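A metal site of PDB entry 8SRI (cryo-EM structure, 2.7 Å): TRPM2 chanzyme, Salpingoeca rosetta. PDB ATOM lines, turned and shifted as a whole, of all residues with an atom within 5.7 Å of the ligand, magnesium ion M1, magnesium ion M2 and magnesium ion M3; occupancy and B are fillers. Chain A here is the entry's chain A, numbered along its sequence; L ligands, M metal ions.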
ATOM      1  N   TRP A1264      14.800  29.055  -0.822  1.00  0.00           N
ATOM      2  CA  TRP A1264      13.789  28.183  -0.243  1.00  0.00           C
ATOM      3  C   TRP A1264      12.426  28.317  -0.912  1.00  0.00           C
ATOM      4  O   TRP A1264      11.454  27.744  -0.430  1.00  0.00           O
ATOM      5  CB  TRP A1264      13.636  28.473   1.264  1.00  0.00           C
ATOM      6  CG  TRP A1264      13.618  29.949   1.627  1.00  0.00           C
ATOM      7  CD1 TRP A1264      14.695  30.734   1.983  1.00  0.00           C
ATOM      8  CD2 TRP A1264      12.485  30.834   1.640  1.00  0.00           C
ATOM      9  NE1 TRP A1264      14.296  32.018   2.228  1.00  0.00           N
ATOM     10  CE2 TRP A1264      12.938  32.114   2.023  1.00  0.00           C
ATOM     11  CE3 TRP A1264      11.114  30.656   1.369  1.00  0.00           C
ATOM     12  CZ2 TRP A1264      12.084  33.211   2.137  1.00  0.00           C
ATOM     13  CZ3 TRP A1264      10.253  31.748   1.488  1.00  0.00           C
ATOM     14  CH2 TRP A1264      10.749  33.013   1.872  1.00  0.00           C
ATOM     15  N   LEU A1319       2.522  34.450   1.481  1.00  0.00           N
ATOM     16  CA  LEU A1319       3.792  34.477   2.187  1.00  0.00           C
ATOM     17  C   LEU A1319       4.530  33.145   2.157  1.00  0.00           C
ATOM     18  O   LEU A1319       5.691  33.084   2.605  1.00  0.00           O
ATOM     19  CB  LEU A1319       3.582  34.872   3.651  1.00  0.00           C
ATOM     20  CG  LEU A1319       3.623  36.355   4.022  1.00  0.00           C
ATOM     21  CD1 LEU A1319       3.045  36.543   5.412  1.00  0.00           C
ATOM     22  CD2 LEU A1319       5.036  36.903   3.949  1.00  0.00           C
ATOM     23  N   LEU A1320       3.920  32.087   1.643  1.00  0.00           N
ATOM     24  CA  LEU A1320       4.517  30.765   1.634  1.00  0.00           C
ATOM     25  C   LEU A1320       5.328  30.571   0.359  1.00  0.00           C
ATOM     26  O   LEU A1320       4.874  30.921  -0.737  1.00  0.00           O
ATOM     27  CB  LEU A1320       3.441  29.690   1.780  1.00  0.00           C
ATOM     28  CG  LEU A1320       2.610  29.769   3.059  1.00  0.00           C
ATOM     29  CD1 LEU A1320       1.580  28.656   3.099  1.00  0.00           C
ATOM     30  CD2 LEU A1320       3.479  29.711   4.311  1.00  0.00           C
ATOM     31  N   GLY A1321       6.518  29.998   0.499  1.00  0.00           N
ATOM     32  CA  GLY A1321       7.454  29.920  -0.610  1.00  0.00           C
ATOM     33  C   GLY A1321       7.269  28.733  -1.531  1.00  0.00           C
ATOM     34  O   GLY A1321       7.705  28.780  -2.681  1.00  0.00           O
ATOM     35  N   LYS A1322       6.625  27.673  -1.048  1.00  0.00           N
ATOM     36  CA  LYS A1322       6.497  26.432  -1.803  1.00  0.00           C
ATOM     37  C   LYS A1322       5.047  26.197  -2.191  1.00  0.00           C
ATOM     38  O   LYS A1322       4.139  26.418  -1.379  1.00  0.00           O
ATOM     39  CB  LYS A1322       7.028  25.247  -0.990  1.00  0.00           C
ATOM     40  N   ASN A1326       3.304  22.848   2.476  1.00  0.00           N
ATOM     41  CA  ASN A1326       4.476  23.262   3.223  1.00  0.00           C
ATOM     42  C   ASN A1326       4.535  22.398   4.475  1.00  0.00           C
ATOM     43  O   ASN A1326       3.699  22.534   5.374  1.00  0.00           O
ATOM     44  CB  ASN A1326       4.395  24.736   3.599  1.00  0.00           C
ATOM     45  CG  ASN A1326       4.726  25.654   2.441  1.00  0.00           C
ATOM     46  OD1 ASN A1326       5.895  25.863   2.124  1.00  0.00           O
ATOM     47  ND2 ASN A1326       3.701  26.192   1.802  1.00  0.00           N
ATOM     48  N   ALA A1328       5.720  21.475   7.910  1.00  0.00           N
ATOM     49  CA  ALA A1328       6.303  22.116   9.070  1.00  0.00           C
ATOM     50  C   ALA A1328       6.541  21.087  10.152  1.00  0.00           C
ATOM     51  O   ALA A1328       5.837  20.071  10.226  1.00  0.00           O
ATOM     52  CB  ALA A1328       5.393  23.228   9.603  1.00  0.00           C
ATOM     53  N   ALA A1329       7.562  21.328  10.964  1.00  0.00           N
ATOM     54  CA  ALA A1329       7.854  20.472  12.096  1.00  0.00           C
ATOM     55  C   ALA A1329       7.762  21.305  13.361  1.00  0.00           C
ATOM     56  O   ALA A1329       8.351  22.395  13.442  1.00  0.00           O
ATOM     57  CB  ALA A1329       9.253  19.858  11.982  1.00  0.00           C
ATOM     58  N   ASP A1330       6.998  20.805  14.330  1.00  0.00           N
ATOM     59  CA  ASP A1330       6.855  21.437  15.623  1.00  0.00           C
ATOM     60  C   ASP A1330       7.476  20.572  16.709  1.00  0.00           C
ATOM     61  O   ASP A1330       7.368  19.340  16.683  1.00  0.00           O
ATOM     62  CB  ASP A1330       5.386  21.714  15.935  1.00  0.00           C
ATOM     63  CG  ASP A1330       4.775  22.699  14.963  1.00  0.00           C
ATOM     64  OD1 ASP A1330       5.386  23.765  14.733  1.00  0.00           O
ATOM     65  OD2 ASP A1330       3.692  22.419  14.414  1.00  0.00           O
ATOM     66  N   ILE A1358       7.200  30.012  22.707  1.00  0.00           N
ATOM     67  CA  ILE A1358       7.905  31.191  22.198  1.00  0.00           C
ATOM     68  C   ILE A1358       6.918  32.261  21.734  1.00  0.00           C
ATOM     69  O   ILE A1358       5.785  31.970  21.333  1.00  0.00           O
ATOM     70  CB  ILE A1358       8.923  30.817  21.090  1.00  0.00           C
ATOM     71  CG1 ILE A1358       8.226  30.235  19.856  1.00  0.00           C
ATOM     72  CG2 ILE A1358      10.047  29.958  21.659  1.00  0.00           C
ATOM     73  CD1 ILE A1358       8.935  30.433  18.560  1.00  0.00           C
ATOM     74  N   ARG A1360       6.135  34.969  19.034  1.00  0.00           N
ATOM     75  CA  ARG A1360       6.423  35.238  17.620  1.00  0.00           C
ATOM     76  C   ARG A1360       6.730  36.710  17.351  1.00  0.00           C
ATOM     77  O   ARG A1360       6.209  37.600  18.030  1.00  0.00           O
ATOM     78  CB  ARG A1360       5.264  34.772  16.747  1.00  0.00           C
ATOM     79  CG  ARG A1360       4.939  33.296  16.903  1.00  0.00           C
ATOM     80  CD  ARG A1360       3.786  32.872  16.003  1.00  0.00           C
ATOM     81  NE  ARG A1360       3.991  33.262  14.613  1.00  0.00           N
ATOM     82  CZ  ARG A1360       4.656  32.535  13.721  1.00  0.00           C
ATOM     83  NH1 ARG A1360       5.197  31.372  14.029  1.00  0.00           N
ATOM     84  NH2 ARG A1360       4.772  32.992  12.473  1.00  0.00           N
ATOM     85  N   ILE A1368       4.098  27.275  19.741  1.00  0.00           N
ATOM     86  CA  ILE A1368       5.068  26.175  19.832  1.00  0.00           C
ATOM     87  C   ILE A1368       6.212  26.445  18.861  1.00  0.00           C
ATOM     88  O   ILE A1368       5.949  26.990  17.762  1.00  0.00           O
ATOM     89  CB  ILE A1368       4.372  24.827  19.526  1.00  0.00           C
ATOM     90  CG1 ILE A1368       3.423  24.418  20.653  1.00  0.00           C
ATOM     91  CG2 ILE A1368       5.308  23.641  19.237  1.00  0.00           C
ATOM     92  CD1 ILE A1368       2.456  23.324  20.302  1.00  0.00           C
ATOM     93  N   PRO A1369       7.493  26.278  19.292  1.00  0.00           N
ATOM     94  CA  PRO A1369       8.642  26.401  18.364  1.00  0.00           C
ATOM     95  C   PRO A1369       8.598  25.391  17.223  1.00  0.00           C
ATOM     96  O   PRO A1369       8.211  24.231  17.409  1.00  0.00           O
ATOM     97  CB  PRO A1369       9.853  26.119  19.274  1.00  0.00           C
ATOM     98  CG  PRO A1369       9.389  26.375  20.634  1.00  0.00           C
ATOM     99  CD  PRO A1369       7.940  26.035  20.669  1.00  0.00           C
ATOM    100  N   GLY A1370       8.989  25.837  16.037  1.00  0.00           N
ATOM    101  CA  GLY A1370       8.959  24.960  14.882  1.00  0.00           C
ATOM    102  C   GLY A1370       9.149  25.750  13.603  1.00  0.00           C
ATOM    103  O   GLY A1370       9.184  26.987  13.616  1.00  0.00           O
ATOM    104  N   GLY A1371       9.266  25.015  12.511  1.00  0.00           N
ATOM    105  CA  GLY A1371       9.501  25.691  11.247  1.00  0.00           C
ATOM    106  C   GLY A1371       9.425  24.786  10.035  1.00  0.00           C
ATOM    107  O   GLY A1371       9.229  23.571  10.135  1.00  0.00           O
ATOM    108  N   PHE A1372       9.525  25.448   8.878  1.00  0.00           N
ATOM    109  CA  PHE A1372       9.428  24.817   7.559  1.00  0.00           C
ATOM    110  C   PHE A1372      10.652  23.933   7.300  1.00  0.00           C
ATOM    111  O   PHE A1372      11.767  24.254   7.711  1.00  0.00           O
ATOM    112  CB  PHE A1372       9.282  25.896   6.499  1.00  0.00           C
ATOM    113  CG  PHE A1372       8.001  26.675   6.618  1.00  0.00           C
ATOM    114  CD1 PHE A1372       6.778  26.086   6.264  1.00  0.00           C
ATOM    115  CD2 PHE A1372       8.015  27.970   7.171  1.00  0.00           C
ATOM    116  CE1 PHE A1372       5.576  26.806   6.405  1.00  0.00           C
ATOM    117  CE2 PHE A1372       6.822  28.689   7.323  1.00  0.00           C
ATOM    118  CZ  PHE A1372       5.602  28.107   6.940  1.00  0.00           C
ATOM    119  N   VAL A1373      10.429  22.805   6.625  1.00  0.00           N
ATOM    120  CA  VAL A1373      11.534  21.887   6.303  1.00  0.00           C
ATOM    121  C   VAL A1373      12.426  22.404   5.179  1.00  0.00           C
ATOM    122  O   VAL A1373      11.957  22.863   4.126  1.00  0.00           O
ATOM    123  CB  VAL A1373      11.029  20.441   6.070  1.00  0.00           C
ATOM    124  CG1 VAL A1373      10.447  19.886   7.360  1.00  0.00           C
ATOM    125  CG2 VAL A1373      10.016  20.281   4.944  1.00  0.00           C
ATOM    126  N   ARG A1385      16.728  21.688  15.176  1.00  0.00           N
ATOM    127  CA  ARG A1385      17.417  22.910  14.738  1.00  0.00           C
ATOM    128  C   ARG A1385      16.593  24.161  15.073  1.00  0.00           C
ATOM    129  O   ARG A1385      17.154  25.168  15.521  1.00  0.00           O
ATOM    130  CB  ARG A1385      17.735  22.823  13.241  1.00  0.00           C
ATOM    131  CG  ARG A1385      18.522  24.006  12.666  1.00  0.00           C
ATOM    132  CD  ARG A1385      18.743  23.897  11.153  1.00  0.00           C
ATOM    133  NE  ARG A1385      17.564  23.489  10.403  1.00  0.00           N
ATOM    134  CZ  ARG A1385      16.592  24.305   9.999  1.00  0.00           C
ATOM    135  NH1 ARG A1385      16.613  25.599  10.265  1.00  0.00           N
ATOM    136  NH2 ARG A1385      15.580  23.808   9.297  1.00  0.00           N
ATOM    137  N   GLU A1386      15.267  24.101  14.816  1.00  0.00           N
ATOM    138  CA  GLU A1386      14.346  25.196  15.146  1.00  0.00           C
ATOM    139  C   GLU A1386      14.223  25.368  16.661  1.00  0.00           C
ATOM    140  O   GLU A1386      13.974  26.497  17.106  1.00  0.00           O
ATOM    141  CB  GLU A1386      12.963  25.041  14.506  1.00  0.00           C
ATOM    142  CG  GLU A1386      12.870  25.256  12.971  1.00  0.00           C
ATOM    143  CD  GLU A1386      13.461  26.572  12.459  1.00  0.00           C
ATOM    144  OE1 GLU A1386      13.242  27.636  13.080  1.00  0.00           O
ATOM    145  OE2 GLU A1386      14.152  26.530  11.422  1.00  0.00           O
ATOM    146  N   GLU A1390      15.290  28.913  18.037  1.00  0.00           N
ATOM    147  CA  GLU A1390      14.228  29.789  18.519  1.00  0.00           C
ATOM    148  C   GLU A1390      14.136  29.860  20.043  1.00  0.00           C
ATOM    149  O   GLU A1390      14.162  30.944  20.617  1.00  0.00           O
ATOM    150  CB  GLU A1390      12.901  29.345  17.892  1.00  0.00           C
ATOM    151  CG  GLU A1390      12.841  29.575  16.377  1.00  0.00           C
ATOM    152  CD  GLU A1390      11.543  29.104  15.761  1.00  0.00           C
ATOM    153  OE1 GLU A1390      10.730  28.472  16.464  1.00  0.00           O
ATOM    154  OE2 GLU A1390      11.320  29.391  14.565  1.00  0.00           O
ATOM    155  N   CYS A1424      -2.761  22.442   9.374  1.00  0.00           N
ATOM    156  CA  CYS A1424      -2.784  23.662  10.183  1.00  0.00           C
ATOM    157  C   CYS A1424      -3.909  24.609   9.798  1.00  0.00           C
ATOM    158  O   CYS A1424      -4.163  24.834   8.610  1.00  0.00           O
ATOM    159  CB  CYS A1424      -1.480  24.465  10.044  1.00  0.00           C
ATOM    160  SG  CYS A1424       0.006  23.831  10.785  1.00  0.00           S
ATOM    161  N   ASP A1426      -3.685  27.825   9.966  1.00  0.00           N
ATOM    162  CA  ASP A1426      -2.720  28.909   9.883  1.00  0.00           C
ATOM    163  C   ASP A1426      -3.313  30.053   9.060  1.00  0.00           C
ATOM    164  O   ASP A1426      -3.865  29.793   7.991  1.00  0.00           O
ATOM    165  CB  ASP A1426      -1.445  28.365   9.214  1.00  0.00           C
ATOM    166  CG  ASP A1426      -0.227  29.267   9.362  1.00  0.00           C
ATOM    167  OD1 ASP A1426      -0.156  30.374   8.769  1.00  0.00           O
ATOM    168  OD2 ASP A1426       0.720  28.836  10.057  1.00  0.00           O
ATOM    169  N   ARG A1428      -1.927  32.404   7.287  1.00  0.00           N
ATOM    170  CA  ARG A1428      -1.209  32.684   6.057  1.00  0.00           C
ATOM    171  C   ARG A1428      -1.543  31.724   4.917  1.00  0.00           C
ATOM    172  O   ARG A1428      -0.962  31.878   3.828  1.00  0.00           O
ATOM    173  CB  ARG A1428       0.310  32.656   6.297  1.00  0.00           C
ATOM    174  CG  ARG A1428       0.795  33.573   7.412  1.00  0.00           C
ATOM    175  CD  ARG A1428       2.199  33.200   7.840  1.00  0.00           C
ATOM    176  NE  ARG A1428       2.236  31.950   8.585  1.00  0.00           N
ATOM    177  CZ  ARG A1428       3.336  31.419   9.110  1.00  0.00           C
ATOM    178  NH1 ARG A1428       4.509  32.009   8.996  1.00  0.00           N
ATOM    179  NH2 ARG A1428       3.252  30.262   9.772  1.00  0.00           N
ATOM    180  N   VAL A1435      -0.031  25.009   5.004  1.00  0.00           N
ATOM    181  CA  VAL A1435       0.897  24.419   5.968  1.00  0.00           C
ATOM    182  C   VAL A1435       0.295  23.146   6.576  1.00  0.00           C
ATOM    183  O   VAL A1435      -0.866  23.145   7.001  1.00  0.00           O
ATOM    184  CB  VAL A1435       1.250  25.445   7.064  1.00  0.00           C
ATOM    185  CG1 VAL A1435       2.318  24.932   8.025  1.00  0.00           C
ATOM    186  CG2 VAL A1435       1.720  26.746   6.429  1.00  0.00           C
ATOM    187  N   THR A1437       1.513  20.120   9.437  1.00  0.00           N
ATOM    188  CA  THR A1437       2.525  19.983  10.485  1.00  0.00           C
ATOM    189  C   THR A1437       2.689  18.532  10.926  1.00  0.00           C
ATOM    190  O   THR A1437       1.759  17.715  10.847  1.00  0.00           O
ATOM    191  CB  THR A1437       2.224  20.867  11.723  1.00  0.00           C
ATOM    192  OG1 THR A1437       3.221  20.630  12.717  1.00  0.00           O
ATOM    193  CG2 THR A1437       0.857  20.573  12.370  1.00  0.00           C
ATOM    194  N   ASP A1459      16.416  34.172  17.037  1.00  0.00           N
ATOM    195  CA  ASP A1459      15.934  34.123  15.645  1.00  0.00           C
ATOM    196  C   ASP A1459      14.607  34.873  15.517  1.00  0.00           C
ATOM    197  O   ASP A1459      14.556  36.082  15.730  1.00  0.00           O
ATOM    198  CB  ASP A1459      15.846  32.686  15.135  1.00  0.00           C
ATOM    199  N   ASP A1460      13.542  34.127  15.182  1.00  0.00           N
ATOM    200  CA  ASP A1460      12.191  34.721  14.964  1.00  0.00           C
ATOM    201  C   ASP A1460      11.336  34.582  16.228  1.00  0.00           C
ATOM    202  O   ASP A1460      10.118  34.444  16.094  1.00  0.00           O
ATOM    203  CB  ASP A1460      11.494  34.091  13.760  1.00  0.00           C
ATOM    204  CG  ASP A1460      11.434  32.581  13.791  1.00  0.00           C
ATOM    205  OD1 ASP A1460      12.421  31.943  13.377  1.00  0.00           O
ATOM    206  OD2 ASP A1460      10.393  32.050  14.224  1.00  0.00           O
ATOM    207  N   PHE A1476      -1.068  30.337  18.375  1.00  0.00           N
ATOM    208  CA  PHE A1476      -1.048  30.529  16.929  1.00  0.00           C
ATOM    209  C   PHE A1476      -1.363  29.204  16.249  1.00  0.00           C
ATOM    210  O   PHE A1476      -0.858  28.164  16.691  1.00  0.00           O
ATOM    211  CB  PHE A1476       0.329  31.075  16.529  1.00  0.00           C
ATOM    212  CG  PHE A1476       0.594  31.081  15.067  1.00  0.00           C
ATOM    213  CD1 PHE A1476      -0.120  31.945  14.226  1.00  0.00           C
ATOM    214  CD2 PHE A1476       1.606  30.264  14.522  1.00  0.00           C
ATOM    215  CE1 PHE A1476       0.131  31.988  12.851  1.00  0.00           C
ATOM    216  CE2 PHE A1476       1.870  30.289  13.144  1.00  0.00           C
ATOM    217  CZ  PHE A1476       1.131  31.160  12.316  1.00  0.00           C
ATOM    218  N   ALA A1477      -2.149  29.264  15.158  1.00  0.00           N
ATOM    219  CA  ALA A1477      -2.554  28.181  14.214  1.00  0.00           C
ATOM    220  C   ALA A1477      -3.267  27.051  14.981  1.00  0.00           C
ATOM    221  O   ALA A1477      -4.141  27.344  15.801  1.00  0.00           O
ATOM    222  CB  ALA A1477      -1.349  27.750  13.369  1.00  0.00           C
ATOM    223  N   HIS A1479      -1.995  24.862  17.241  1.00  0.00           N
ATOM    224  CA  HIS A1479      -1.142  24.380  18.331  1.00  0.00           C
ATOM    225  C   HIS A1479      -1.916  23.883  19.563  1.00  0.00           C
ATOM    226  O   HIS A1479      -1.342  23.120  20.344  1.00  0.00           O
ATOM    227  CB  HIS A1479      -0.167  25.497  18.679  1.00  0.00           C
ATOM    228  CG  HIS A1479       0.899  25.701  17.645  1.00  0.00           C
ATOM    229  ND1 HIS A1479       1.803  26.730  17.704  1.00  0.00           N
ATOM    230  CD2 HIS A1479       1.200  24.990  16.526  1.00  0.00           C
ATOM    231  CE1 HIS A1479       2.615  26.668  16.669  1.00  0.00           C
ATOM    232  NE2 HIS A1479       2.273  25.615  15.933  1.00  0.00           N
ATOM    233  N   LEU A1482      -2.472  20.297  18.783  1.00  0.00           N
ATOM    234  CA  LEU A1482      -1.188  19.619  19.018  1.00  0.00           C
ATOM    235  C   LEU A1482      -0.940  19.355  20.506  1.00  0.00           C
ATOM    236  O   LEU A1482      -0.462  18.273  20.883  1.00  0.00           O
ATOM    237  CB  LEU A1482      -0.051  20.454  18.425  1.00  0.00           C
ATOM    238  CG  LEU A1482      -0.061  20.594  16.897  1.00  0.00           C
ATOM    239  CD1 LEU A1482       1.170  21.357  16.439  1.00  0.00           C
ATOM    240  CD2 LEU A1482      -0.163  19.252  16.164  1.00  0.00           C
HETATM  241  N1  LIG L   1       7.394  29.245   3.482  1.00  0.00           N
HETATM  242  C1  LIG L   1       7.529  30.404   4.132  1.00  0.00           C
HETATM  243  N2  LIG L   1       8.664  30.799   4.742  1.00  0.00           N
HETATM  244  C2  LIG L   1       9.775  30.026   4.723  1.00  0.00           C
HETATM  245  C3  LIG L   1       9.696  28.738   4.023  1.00  0.00           C
HETATM  246  C4  LIG L   1       8.421  28.378   3.382  1.00  0.00           C
HETATM  247  N3  LIG L   1       8.283  27.208   2.716  1.00  0.00           N
HETATM  248  N4  LIG L   1      10.896  28.154   4.145  1.00  0.00           N
HETATM  249  C5  LIG L   1      11.681  28.991   4.858  1.00  0.00           C
HETATM  250  N5  LIG L   1      11.022  30.108   5.209  1.00  0.00           N
HETATM  251  C6  LIG L   1      11.669  31.182   6.004  1.00  0.00           C
HETATM  252  C7  LIG L   1      10.998  32.542   5.849  1.00  0.00           C
HETATM  253  O1  LIG L   1      11.958  33.476   5.372  1.00  0.00           O
HETATM  254  C8  LIG L   1      10.561  32.947   7.232  1.00  0.00           C
HETATM  255  O2  LIG L   1      10.861  34.321   7.466  1.00  0.00           O
HETATM  256  O3  LIG L   1      11.635  30.878   7.404  1.00  0.00           O
HETATM  257  C9  LIG L   1      11.385  32.065   8.146  1.00  0.00           C
HETATM  258  C10 LIG L   1      10.664  31.769   9.457  1.00  0.00           C
HETATM  259  O4  LIG L   1      11.273  30.658  10.090  1.00  0.00           O
HETATM  260  P1  LIG L   1      10.344  29.409  10.471  1.00  0.00           P
HETATM  261  O5  LIG L   1      10.705  29.002  11.871  1.00  0.00           O
HETATM  262  O6  LIG L   1      10.439  28.406   9.347  1.00  0.00           O
HETATM  263  O7  LIG L   1       8.882  30.106  10.425  1.00  0.00           O
HETATM  264  P2  LIG L   1       7.725  29.888  11.522  1.00  0.00           P
HETATM  265  O8  LIG L   1       6.555  30.747  11.117  1.00  0.00           O
HETATM  266  O9  LIG L   1       8.297  30.023  12.914  1.00  0.00           O
HETATM  267  O10 LIG L   1       7.309  28.359  11.298  1.00  0.00           O
HETATM  268  C11 LIG L   1       6.022  28.038  10.790  1.00  0.00           C
HETATM  269  O11 LIG L   1       3.718  27.993  11.486  1.00  0.00           O
HETATM  270  O12 LIG L   1       1.929  26.563  10.915  1.00  0.00           O
HETATM  271  C12 LIG L   1       2.891  26.908  11.912  1.00  0.00           C
HETATM  272  O13 LIG L   1       3.349  24.937  13.167  1.00  0.00           O
HETATM  273  C13 LIG L   1       3.840  25.751  12.114  1.00  0.00           C
HETATM  274  O14 LIG L   1       5.267  26.453  13.898  1.00  0.00           O
HETATM  275  C14 LIG L   1       5.153  26.397  12.475  1.00  0.00           C
HETATM  276  C15 LIG L   1       5.051  27.815  11.937  1.00  0.00           C
HETATM  277 MG    MG M   1      12.505  29.827  12.672  1.00  0.00          MG
HETATM  278 MG    MG M   2       9.235  29.152  14.528  1.00  0.00          MG
HETATM  279 MG    MG M   3      12.842  29.067  10.730  1.00  0.00          MG
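The side-chain carboxylate (OD2) of Asp 1426 lies within hydrogen-bond range of an oxygen (O12) of the ligand, at 2.7 Å.
OD1 of Asn 1326 sits at hydrogen-bond distance from N3 of the ligand, 2.8 Å away.
O14 of the ligand lies within hydrogen-bond range of OD1 of Asp 1330 (2.8 Å).
An oxygen (O8) of the ligand lies within salt-bridge range of the guanidinium group (NH1) of Arg 1428.
An oxygen (O13) of the ligand sits at hydrogen-bond distance from a ring nitrogen (NE2) of His 1479.
O6 of the ligand lies within hydrogen-bond range of N of Phe 1372 (3.1 Å).
The guanidinium group (NH2) of Arg 1360 lies within salt-bridge range of an oxygen (O8) of the ligand (3.2 Å).
N1 of the ligand lies within hydrogen-bond range of N of Gly 1321 (3.2 Å).
The side-chain sulfur (SG) of Cys 1424 is in hydrogen-bond range of an oxygen (O12) of the ligand (3.3 Å).
The side-chain carboxylate of Glu 1386 lies within salt-bridge range of the guanidinium group of Arg 1385 (2.9 Å).
OD1 of Asp 1426 is in salt-bridge range of NE of Arg 1428 (2.9 Å).
O of Lys 1322 is in hydrogen-bond range of ND2 of Asn 1326 (3.2 Å).
The side-chain hydroxyl (OG1) of Thr 1437 sits at hydrogen-bond distance from the side-chain carboxylate (OD2) of Asp 1330.
The backbone carbonyl oxygen (O) of Phe 1476 lies close to a ring nitrogen (ND1) of His 1479, at 3.2 Å.
A ring nitrogen (ND1) of His 1479 is in hydrogen-bond range of the backbone NH (N) of Ile 1368.
O of Val 1435 lies within hydrogen-bond range of N of Cys 1424 (3.1 Å).
The backbone carbonyl oxygen of Gly 1371 is in hydrogen-bond range of the backbone NH of Ala 1329 (2.9 Å).
Trp 1264 touches the ligand (CZ2 to O1, 3.2 Å).
Leu 1319 touches the ligand.
Leu 1320 touches the ligand (CA to N1, 3.7 Å).
CB of Ala 1328 touches C13 of the ligand, 3.9 Å away.
Ile 1368 touches the ligand (O to O14, 3.96 Å).
Gly 1371 touches the ligand.
Val 1435 touches the ligand (CG1 to O12, 3.3 Å).
Phe 1476 touches the ligand (CE2 to O11, 3.4 Å).
Hydrophobic or aromatic side chains that line the ligand: Trp 1264, Ala 1328, Phe 1372, Val 1435, Phe 1476 and His 1479.
Of the 31 residues printed, 21 come within 4 Å of the ligand.
Of the 31 residues printed, 3 come within 4 Å of magnesium ion M1.
The nearest printed residue that does not touch magnesium ion M1 is Gly 1370 (4.5 Å).
Of the 31 residues printed, 3 come within 4 Å of magnesium ion M2.
The nearest printed residue that does not touch magnesium ion M2 is Ile 1358 (4.2 Å).
Along chain A the residues within 4 Å of magnesium ion M3 span positions 1386 to 1460.
An oxygen (O5) of the ligand binds magnesium ion M1 (2.1 Å).
Magnesium ion M1 is bound by OD1 of Asp 1460, at 2.2 Å.
OE2 of Glu 1390 binds magnesium ion M1, 2.3 Å away.
The side-chain carboxylate (OE1) of Glu 1386 binds magnesium ion M1 (2.3 Å).
Magnesium ion M1 has four donor atoms within binding distance.
O9 of the ligand is bound to magnesium ion M2 (2.1 Å).
Magnesium ion M2 is bound by OE2 of Glu 1390 (2.1 Å).
The backbone carbonyl oxygen (O) of Gly 1370 binds magnesium ion M2, 2.3 Å away.
OE1 of Glu 1390 is bound to magnesium ion M2.
Magnesium ion M2 has four donor atoms within binding distance.
Magnesium ion M3 is bound by O4 of the ligand and O5 of the ligand.
Slightly farther from magnesium ion M3 lies OE1 of Glu 1386 (2.8 Å).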
